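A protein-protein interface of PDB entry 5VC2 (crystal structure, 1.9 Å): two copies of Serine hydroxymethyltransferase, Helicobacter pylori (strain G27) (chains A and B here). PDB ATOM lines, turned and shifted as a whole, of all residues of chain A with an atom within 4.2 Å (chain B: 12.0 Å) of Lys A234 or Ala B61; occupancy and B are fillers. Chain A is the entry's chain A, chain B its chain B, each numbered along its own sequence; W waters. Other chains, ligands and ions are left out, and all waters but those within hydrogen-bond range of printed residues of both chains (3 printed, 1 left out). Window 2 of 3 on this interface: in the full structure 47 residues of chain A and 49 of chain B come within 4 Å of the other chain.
Water W2 lies within hydrogen-bond range of the side-chain carboxylate of Glu A41 (2.6 Å), the backbone carbonyl oxygen of Asn B58 (2.6 Å) and the backbone NH of Asn A42 (3.1 Å). Water W1 lies within hydrogen-bond range of OG1 of Thr B57 (2.7 Å), N of Arg A240 (3.1 Å) and NE2 of His B270 (3.5 Å). Water W3 bridges N of Tyr B60 (3.0 Å) and OE1 of Glu A41 (3.0 Å).
Of chain B, only Asn B58 comes within 4 Å of Asn A42. No residue of chain B comes within 4 Å of Ala A207. No residue of chain B comes within 4 Å of Thr A231. No residue of chain B comes within 4 Å of Thr A235. No residue of chain B comes within 4 Å of Leu A236. Printed residues of chain B within 4 Å of Arg A240: Thr B57 (3.2 Å), Lys B59 (3.2 Å), Tyr B60 (2.4 Å), Ala B61 (3.2 Å), Pro B267 (2.8 Å) and Leu B268 (3.2 Å). Of the printed residues of chain A, Lys B59 touches Arg A240 (3.2 Å). Of the printed residues of chain A, Tyr B60 touches Glu A41 and Arg A240. Ala B61 touches just these residues of chain A: Ser A40 (3.3 Å), Glu A41 (2.9 Å), His A233 (3.6 Å), Lys A234 (3.9 Å) and Arg A240 (3.2 Å). Of the printed residues of chain A, Pro B267 touches Arg A240 (2.8 Å). The nearest printed residue of chain A that does not touch Pro B267 is His A233 (8.7 Å).
Among the printed residues, pairs that only touch across the chains: Arg A240 with Thr B57 (3.2 Å), Arg A240 with Leu B268 (3.2 Å), Ser A40 with Ala B61 (3.3 Å), Asn A42 with Asn B58 (3.5 Å), His A233 with Ala B61 (3.6 Å), Glu A41 with Asn B58 (3.7 Å), Glu A41 with Tyr B60 (3.9 Å) and Lys A234 with Ala B61 (3.9 Å).
The side-chain hydroxyl of Ser A40 lies within hydrogen-bond range of the side-chain carboxylate of Glu A41, 3.2 Å away. The backbone carbonyl oxygen (O) of Lys A234 sits at hydrogen-bond distance from the side-chain amide nitrogen (ND2) of Asn A42 (3.0 Å). The side-chain amino group (NZ) of Lys B59 is in salt-bridge range of the side-chain carboxylate (OD2) of Asp B77, at 2.6 Å. The side-chain carboxylate of Asp B77 sits at hydrogen-bond distance from the side-chain hydroxyl of Tyr B60 (2.8 Å).
No position is printed for both chains. Of the 13 pairs that touch across the chains among the printed residues, none has its exchanged pair printed and touching as well.
N of Ala B61 is in hydrogen-bond range of OE1 of Glu A41 (2.9 Å). NH1 of Arg A240 sits at hydrogen-bond distance from O of Lys B59 (3.2 Å). The backbone carbonyl oxygen of Tyr B60 lies within hydrogen-bond range of the guanidinium group of Arg A240. NH2 of Arg A240 sits at hydrogen-bond distance from O of Pro B267, 2.8 Å away. The guanidinium group (NH1) of Arg A240 sits close to the backbone NH (N) of Ala B61 (3.3 Å).
Printed residues of chain B that touch a printed residue of chain A: Thr B57, Asn B58, Lys B59, Tyr B60, Ala B61, Pro B267 and Leu B268. Hydrophobic or aromatic side chains of chain B within 4 Å of the printed part of chain A: Ala B61 and Leu B268. Printed residues of chain A that touch a printed residue of chain B: Ser A40, Glu A41, Asn A42, His A233, Lys A234 and Arg A240. Hydrophobic or aromatic side chains of chain A that line the printed part of chain B: His A233. Among the printed residues, 13 pairs touch across the chains. Among the printed residues, no Asp or Glu carboxylate lies within 4 Å of a Lys or Arg side-chain nitrogen of the other chain.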
ATOM      1  N   SER A  40      -4.433   2.978  11.469  1.00  0.00           N
ATOM      2  CA  SER A  40      -3.975   2.588  12.798  1.00  0.00           C
ATOM      3  C   SER A  40      -3.857   3.750  13.790  1.00  0.00           C
ATOM      4  O   SER A  40      -3.567   3.508  14.966  1.00  0.00           O
ATOM      5  CB  SER A  40      -2.612   1.905  12.686  1.00  0.00           C
ATOM      6  OG  SER A  40      -1.644   2.839  12.230  1.00  0.00           O
ATOM      7  N   GLU A  41      -4.055   4.995  13.369  1.00  0.00           N
ATOM      8  CA  GLU A  41      -3.836   6.107  14.290  1.00  0.00           C
ATOM      9  C   GLU A  41      -5.143   6.487  14.982  1.00  0.00           C
ATOM     10  O   GLU A  41      -6.240   6.202  14.492  1.00  0.00           O
ATOM     11  CB  GLU A  41      -3.253   7.317  13.556  1.00  0.00           C
ATOM     12  CG  GLU A  41      -1.962   6.990  12.795  1.00  0.00           C
ATOM     13  CD  GLU A  41      -0.851   6.497  13.705  1.00  0.00           C
ATOM     14  OE1 GLU A  41      -0.599   7.151  14.738  1.00  0.00           O
ATOM     15  OE2 GLU A  41      -0.235   5.452  13.392  1.00  0.00           O
ATOM     16  N   ASN A  42      -5.019   7.116  16.147  1.00  0.00           N
ATOM     17  CA  ASN A  42      -6.214   7.531  16.874  1.00  0.00           C
ATOM     18  C   ASN A  42      -5.818   8.563  17.922  1.00  0.00           C
ATOM     19  O   ASN A  42      -4.654   8.956  18.033  1.00  0.00           O
ATOM     20  CB  ASN A  42      -6.929   6.316  17.490  1.00  0.00           C
ATOM     21  CG  ASN A  42      -8.442   6.449  17.439  1.00  0.00           C
ATOM     22  OD1 ASN A  42      -8.969   7.542  17.602  1.00  0.00           O
ATOM     23  ND2 ASN A  42      -9.145   5.336  17.223  1.00  0.00           N
ATOM     24  N   ALA A 207      -5.674  -6.769  16.974  1.00  0.00           N
ATOM     25  CA  ALA A 207      -5.130  -5.432  17.210  1.00  0.00           C
ATOM     26  C   ALA A 207      -5.739  -4.387  16.280  1.00  0.00           C
ATOM     27  O   ALA A 207      -5.911  -3.232  16.676  1.00  0.00           O
ATOM     28  CB  ALA A 207      -3.603  -5.452  17.053  1.00  0.00           C
ATOM     29  N   THR A 231      -3.536  -4.838  20.664  1.00  0.00           N
ATOM     30  CA  THR A 231      -3.065  -3.586  21.222  1.00  0.00           C
ATOM     31  C   THR A 231      -4.166  -2.973  22.085  1.00  0.00           C
ATOM     32  O   THR A 231      -5.338  -3.361  22.007  1.00  0.00           O
ATOM     33  CB  THR A 231      -2.670  -2.617  20.109  1.00  0.00           C
ATOM     34  OG1 THR A 231      -3.762  -2.501  19.184  1.00  0.00           O
ATOM     35  CG2 THR A 231      -1.432  -3.138  19.371  1.00  0.00           C
ATOM     36  N   HIS A 233      -4.194   0.539  22.126  1.00  0.00           N
ATOM     37  CA  HIS A 233      -4.427   1.844  21.500  1.00  0.00           C
ATOM     38  C   HIS A 233      -5.249   1.665  20.217  1.00  0.00           C
ATOM     39  O   HIS A 233      -6.189   0.872  20.216  1.00  0.00           O
ATOM     40  CB  HIS A 233      -3.102   2.590  21.273  1.00  0.00           C
ATOM     41  CG  HIS A 233      -2.019   1.785  20.610  1.00  0.00           C
ATOM     42  ND1 HIS A 233      -1.527   0.606  21.133  1.00  0.00           N
ATOM     43  CD2 HIS A 233      -1.288   2.033  19.495  1.00  0.00           C
ATOM     44  CE1 HIS A 233      -0.564   0.147  20.352  1.00  0.00           C
ATOM     45  NE2 HIS A 233      -0.402   0.992  19.349  1.00  0.00           N
ATOM     46  N   LYS A 234      -4.958   2.399  19.139  1.00  0.00           N
ATOM     47  CA  LYS A 234      -5.661   2.229  17.837  1.00  0.00           C
ATOM     48  C   LYS A 234      -7.169   2.370  18.077  1.00  0.00           C
ATOM     49  O   LYS A 234      -7.581   3.316  18.760  1.00  0.00           O
ATOM     50  CB  LYS A 234      -5.236   0.912  17.186  1.00  0.00           C
ATOM     51  CG  LYS A 234      -3.741   0.833  16.761  1.00  0.00           C
ATOM     52  CD  LYS A 234      -3.470  -0.560  16.156  1.00  0.00           C
ATOM     53  CE  LYS A 234      -2.191  -0.628  15.335  1.00  0.00           C
ATOM     54  NZ  LYS A 234      -1.018  -0.760  16.198  1.00  0.00           N
ATOM     55  N   THR A 235      -8.016   1.437  17.599  1.00  0.00           N
ATOM     56  CA  THR A 235      -9.466   1.662  17.697  1.00  0.00           C
ATOM     57  C   THR A 235     -10.004   1.541  19.120  1.00  0.00           C
ATOM     58  O   THR A 235     -11.171   1.886  19.338  1.00  0.00           O
ATOM     59  CB  THR A 235     -10.265   0.717  16.772  1.00  0.00           C
ATOM     60  OG1 THR A 235     -10.032  -0.664  17.115  1.00  0.00           O
ATOM     61  CG2 THR A 235      -9.909   0.946  15.307  1.00  0.00           C
ATOM     62  N   LEU A 236      -9.204   1.092  20.089  1.00  0.00           N
ATOM     63  CA  LEU A 236      -9.652   1.092  21.484  1.00  0.00           C
ATOM     64  C   LEU A 236      -9.383   2.415  22.189  1.00  0.00           C
ATOM     65  O   LEU A 236      -9.950   2.660  23.259  1.00  0.00           O
ATOM     66  CB  LEU A 236      -8.983  -0.038  22.281  1.00  0.00           C
ATOM     67  CG  LEU A 236      -9.506  -1.455  22.030  1.00  0.00           C
ATOM     68  CD1 LEU A 236      -8.658  -2.463  22.812  1.00  0.00           C
ATOM     69  CD2 LEU A 236     -11.003  -1.597  22.408  1.00  0.00           C
ATOM     70  N   ARG A 237      -8.538   3.268  21.616  1.00  0.00           N
ATOM     71  CA  ARG A 237      -8.248   4.612  22.140  1.00  0.00           C
ATOM     72  C   ARG A 237      -7.634   4.595  23.541  1.00  0.00           C
ATOM     73  O   ARG A 237      -7.674   5.614  24.255  1.00  0.00           O
ATOM     74  CB  ARG A 237      -9.505   5.502  22.130  1.00  0.00           C
ATOM     75  CG  ARG A 237     -10.147   5.648  20.734  1.00  0.00           C
ATOM     76  CD  ARG A 237     -11.310   6.666  20.729  1.00  0.00           C
ATOM     77  NE  ARG A 237     -10.803   7.973  21.114  1.00  0.00           N
ATOM     78  CZ  ARG A 237     -11.531   8.986  21.573  1.00  0.00           C
ATOM     79  NH1 ARG A 237     -12.847   8.871  21.702  1.00  0.00           N
ATOM     80  NH2 ARG A 237     -10.926  10.126  21.910  1.00  0.00           N
ATOM     81  N   ARG A 240      -0.704   3.231  24.620  1.00  0.00           N
ATOM     82  CA  ARG A 240       0.110   2.268  23.879  1.00  0.00           C
ATOM     83  C   ARG A 240       0.436   1.059  24.762  1.00  0.00           C
ATOM     84  O   ARG A 240       0.888   1.205  25.901  1.00  0.00           O
ATOM     85  CB  ARG A 240       1.373   2.945  23.365  1.00  0.00           C
ATOM     86  CG  ARG A 240       1.084   3.665  22.066  1.00  0.00           C
ATOM     87  CD  ARG A 240       1.694   5.023  22.044  1.00  0.00           C
ATOM     88  NE  ARG A 240       2.930   4.994  21.280  1.00  0.00           N
ATOM     89  CZ  ARG A 240       2.987   5.193  19.971  1.00  0.00           C
ATOM     90  NH1 ARG A 240       1.868   5.451  19.296  1.00  0.00           N
ATOM     91  NH2 ARG A 240       4.156   5.143  19.340  1.00  0.00           N
ATOM     92  N   ILE B  55      -0.188  14.825  24.907  1.00  0.00           N
ATOM     93  CA  ILE B  55      -0.756  14.291  23.671  1.00  0.00           C
ATOM     94  C   ILE B  55       0.319  13.617  22.828  1.00  0.00           C
ATOM     95  O   ILE B  55       0.029  13.089  21.750  1.00  0.00           O
ATOM     96  CB  ILE B  55      -1.513  15.378  22.868  1.00  0.00           C
ATOM     97  CG1 ILE B  55      -0.702  16.683  22.684  1.00  0.00           C
ATOM     98  CG2 ILE B  55      -2.804  15.714  23.581  1.00  0.00           C
ATOM     99  CD1 ILE B  55       0.464  16.598  21.726  1.00  0.00           C
ATOM    100  N   LEU B  56       1.572  13.634  23.293  1.00  0.00           N
ATOM    101  CA  LEU B  56       2.615  12.933  22.544  1.00  0.00           C
ATOM    102  C   LEU B  56       2.358  11.437  22.470  1.00  0.00           C
ATOM    103  O   LEU B  56       2.929  10.762  21.606  1.00  0.00           O
ATOM    104  CB  LEU B  56       3.989  13.184  23.164  1.00  0.00           C
ATOM    105  CG  LEU B  56       4.478  14.630  23.112  1.00  0.00           C
ATOM    106  CD1 LEU B  56       5.831  14.725  23.846  1.00  0.00           C
ATOM    107  CD2 LEU B  56       4.615  15.098  21.665  1.00  0.00           C
ATOM    108  N   THR B  57       1.512  10.906  23.349  1.00  0.00           N
ATOM    109  CA  THR B  57       1.154   9.496  23.249  1.00  0.00           C
ATOM    110  C   THR B  57       0.500   9.154  21.910  1.00  0.00           C
ATOM    111  O   THR B  57       0.587   8.000  21.478  1.00  0.00           O
ATOM    112  CB  THR B  57       0.240   9.101  24.410  1.00  0.00           C
ATOM    113  OG1 THR B  57      -0.040   7.702  24.341  1.00  0.00           O
ATOM    114  CG2 THR B  57      -1.052   9.851  24.336  1.00  0.00           C
ATOM    115  N   ASN B  58      -0.123  10.126  21.222  1.00  0.00           N
ATOM    116  CA  ASN B  58      -0.791   9.835  19.949  1.00  0.00           C
ATOM    117  C   ASN B  58       0.144   9.780  18.749  1.00  0.00           C
ATOM    118  O   ASN B  58      -0.318   9.475  17.646  1.00  0.00           O
ATOM    119  CB  ASN B  58      -1.869  10.877  19.654  1.00  0.00           C
ATOM    120  CG  ASN B  58      -2.967  10.857  20.669  1.00  0.00           C
ATOM    121  OD1 ASN B  58      -3.310   9.802  21.190  1.00  0.00           O
ATOM    122  ND2 ASN B  58      -3.517  12.030  20.982  1.00  0.00           N
ATOM    123  N   LYS B  59       1.423  10.082  18.904  1.00  0.00           N
ATOM    124  CA  LYS B  59       2.304  10.177  17.747  1.00  0.00           C
ATOM    125  C   LYS B  59       2.894   8.800  17.439  1.00  0.00           C
ATOM    126  O   LYS B  59       3.380   8.116  18.345  1.00  0.00           O
ATOM    127  CB  LYS B  59       3.392  11.221  18.011  1.00  0.00           C
ATOM    128  CG  LYS B  59       3.869  11.922  16.754  1.00  0.00           C
ATOM    129  CD  LYS B  59       5.004  12.875  17.049  1.00  0.00           C
ATOM    130  CE  LYS B  59       5.501  13.531  15.763  1.00  0.00           C
ATOM    131  NZ  LYS B  59       6.722  14.352  15.983  1.00  0.00           N
ATOM    132  N   TYR B  60       2.797   8.379  16.171  1.00  0.00           N
ATOM    133  CA  TYR B  60       3.318   7.100  15.668  1.00  0.00           C
ATOM    134  C   TYR B  60       2.721   5.837  16.299  1.00  0.00           C
ATOM    135  O   TYR B  60       3.417   5.144  17.047  1.00  0.00           O
ATOM    136  CB  TYR B  60       4.833   7.018  15.863  1.00  0.00           C
ATOM    137  CG  TYR B  60       5.618   8.214  15.405  1.00  0.00           C
ATOM    138  CD1 TYR B  60       5.396   8.783  14.156  1.00  0.00           C
ATOM    139  CD2 TYR B  60       6.591   8.776  16.231  1.00  0.00           C
ATOM    140  CE1 TYR B  60       6.135   9.884  13.733  1.00  0.00           C
ATOM    141  CE2 TYR B  60       7.332   9.876  15.826  1.00  0.00           C
ATOM    142  CZ  TYR B  60       7.106  10.427  14.578  1.00  0.00           C
ATOM    143  OH  TYR B  60       7.851  11.520  14.185  1.00  0.00           O
ATOM    144  N   ALA B  61       1.476   5.479  15.970  1.00  0.00           N
ATOM    145  CA  ALA B  61       0.892   4.225  16.485  1.00  0.00           C
ATOM    146  C   ALA B  61       1.575   2.977  15.909  1.00  0.00           C
ATOM    147  O   ALA B  61       1.733   1.962  16.603  1.00  0.00           O
ATOM    148  CB  ALA B  61      -0.628   4.170  16.207  1.00  0.00           C
ATOM    149  N   ASP B  77      12.987  11.627  15.354  1.00  0.00           N
ATOM    150  CA  ASP B  77      12.156  12.737  15.807  1.00  0.00           C
ATOM    151  C   ASP B  77      13.003  13.776  16.538  1.00  0.00           C
ATOM    152  O   ASP B  77      13.976  13.447  17.218  1.00  0.00           O
ATOM    153  CB  ASP B  77      11.045  12.205  16.726  1.00  0.00           C
ATOM    154  CG  ASP B  77       9.881  13.177  16.898  1.00  0.00           C
ATOM    155  OD1 ASP B  77      10.054  14.247  17.526  1.00  0.00           O
ATOM    156  OD2 ASP B  77       8.772  12.855  16.412  1.00  0.00           O
ATOM    157  N   HIS B 101      13.736   0.333  27.747  1.00  0.00           N
ATOM    158  CA  HIS B 101      12.571   0.525  28.604  1.00  0.00           C
ATOM    159  C   HIS B 101      12.884   0.397  30.091  1.00  0.00           C
ATOM    160  O   HIS B 101      12.019   0.723  30.911  1.00  0.00           O
ATOM    161  CB  HIS B 101      11.466  -0.472  28.232  1.00  0.00           C
ATOM    162  CG  HIS B 101      10.714  -0.106  26.989  1.00  0.00           C
ATOM    163  ND1 HIS B 101      11.176  -0.403  25.724  1.00  0.00           N
ATOM    164  CD2 HIS B 101       9.533   0.533  26.818  1.00  0.00           C
ATOM    165  CE1 HIS B 101      10.310   0.038  24.827  1.00  0.00           C
ATOM    166  NE2 HIS B 101       9.305   0.610  25.465  1.00  0.00           N
ATOM    167  N   GLY B 266       8.377   0.406  18.251  1.00  0.00           N
ATOM    168  CA  GLY B 266       7.385   1.366  18.709  1.00  0.00           C
ATOM    169  C   GLY B 266       7.967   2.449  19.599  1.00  0.00           C
ATOM    170  O   GLY B 266       8.222   2.215  20.786  1.00  0.00           O
ATOM    171  N   PRO B 267       8.164   3.642  19.036  1.00  0.00           N
ATOM    172  CA  PRO B 267       8.767   4.751  19.793  1.00  0.00           C
ATOM    173  C   PRO B 267       7.700   5.499  20.580  1.00  0.00           C
ATOM    174  O   PRO B 267       6.723   5.997  20.018  1.00  0.00           O
ATOM    175  CB  PRO B 267       9.385   5.628  18.699  1.00  0.00           C
ATOM    176  CG  PRO B 267       8.608   5.274  17.424  1.00  0.00           C
ATOM    177  CD  PRO B 267       7.739   4.066  17.692  1.00  0.00           C
ATOM    178  N   LEU B 268       7.883   5.561  21.891  1.00  0.00           N
ATOM    179  CA  LEU B 268       6.915   6.174  22.793  1.00  0.00           C
ATOM    180  C   LEU B 268       7.380   7.608  23.011  1.00  0.00           C
ATOM    181  O   LEU B 268       8.264   7.864  23.832  1.00  0.00           O
ATOM    182  CB  LEU B 268       6.829   5.390  24.099  1.00  0.00           C
ATOM    183  CG  LEU B 268       6.399   3.913  23.983  1.00  0.00           C
ATOM    184  CD1 LEU B 268       6.528   3.197  25.326  1.00  0.00           C
ATOM    185  CD2 LEU B 268       5.004   3.779  23.452  1.00  0.00           C
ATOM    186  N   MET B 269       6.808   8.542  22.246  1.00  0.00           N
ATOM    187  CA  MET B 269       7.351   9.899  22.247  1.00  0.00           C
ATOM    188  C   MET B 269       7.077  10.624  23.559  1.00  0.00           C
ATOM    189  O   MET B 269       7.851  11.512  23.954  1.00  0.00           O
ATOM    190  CB  MET B 269       6.784  10.701  21.068  1.00  0.00           C
ATOM    191  CG  MET B 269       7.135  10.130  19.701  1.00  0.00           C
ATOM    192  SD  MET B 269       8.893   9.722  19.547  1.00  0.00           S
ATOM    193  CE  MET B 269       9.666  11.235  20.041  1.00  0.00           C
ATOM    194  N   HIS B 270       5.978  10.293  24.239  1.00  0.00           N
ATOM    195  CA  HIS B 270       5.759  10.888  25.553  1.00  0.00           C
ATOM    196  C   HIS B 270       6.831  10.446  26.547  1.00  0.00           C
ATOM    197  O   HIS B 270       7.280  11.247  27.375  1.00  0.00           O
ATOM    198  CB  HIS B 270       4.359  10.553  26.059  1.00  0.00           C
ATOM    199  CG  HIS B 270       4.052   9.085  26.062  1.00  0.00           C
ATOM    200  ND1 HIS B 270       3.999   8.334  24.909  1.00  0.00           N
ATOM    201  CD2 HIS B 270       3.751   8.240  27.076  1.00  0.00           C
ATOM    202  CE1 HIS B 270       3.692   7.086  25.212  1.00  0.00           C
ATOM    203  NE2 HIS B 270       3.536   7.001  26.519  1.00  0.00           N
HETATM  204  O   HOH W   1       0.360   5.692  26.080  1.00  0.00           O
HETATM  205  O   HOH W   2      -2.019   7.615  16.852  1.00  0.00           O
HETATM  206  O   HOH W   3       1.315   9.221  13.759  1.00  0.00           O
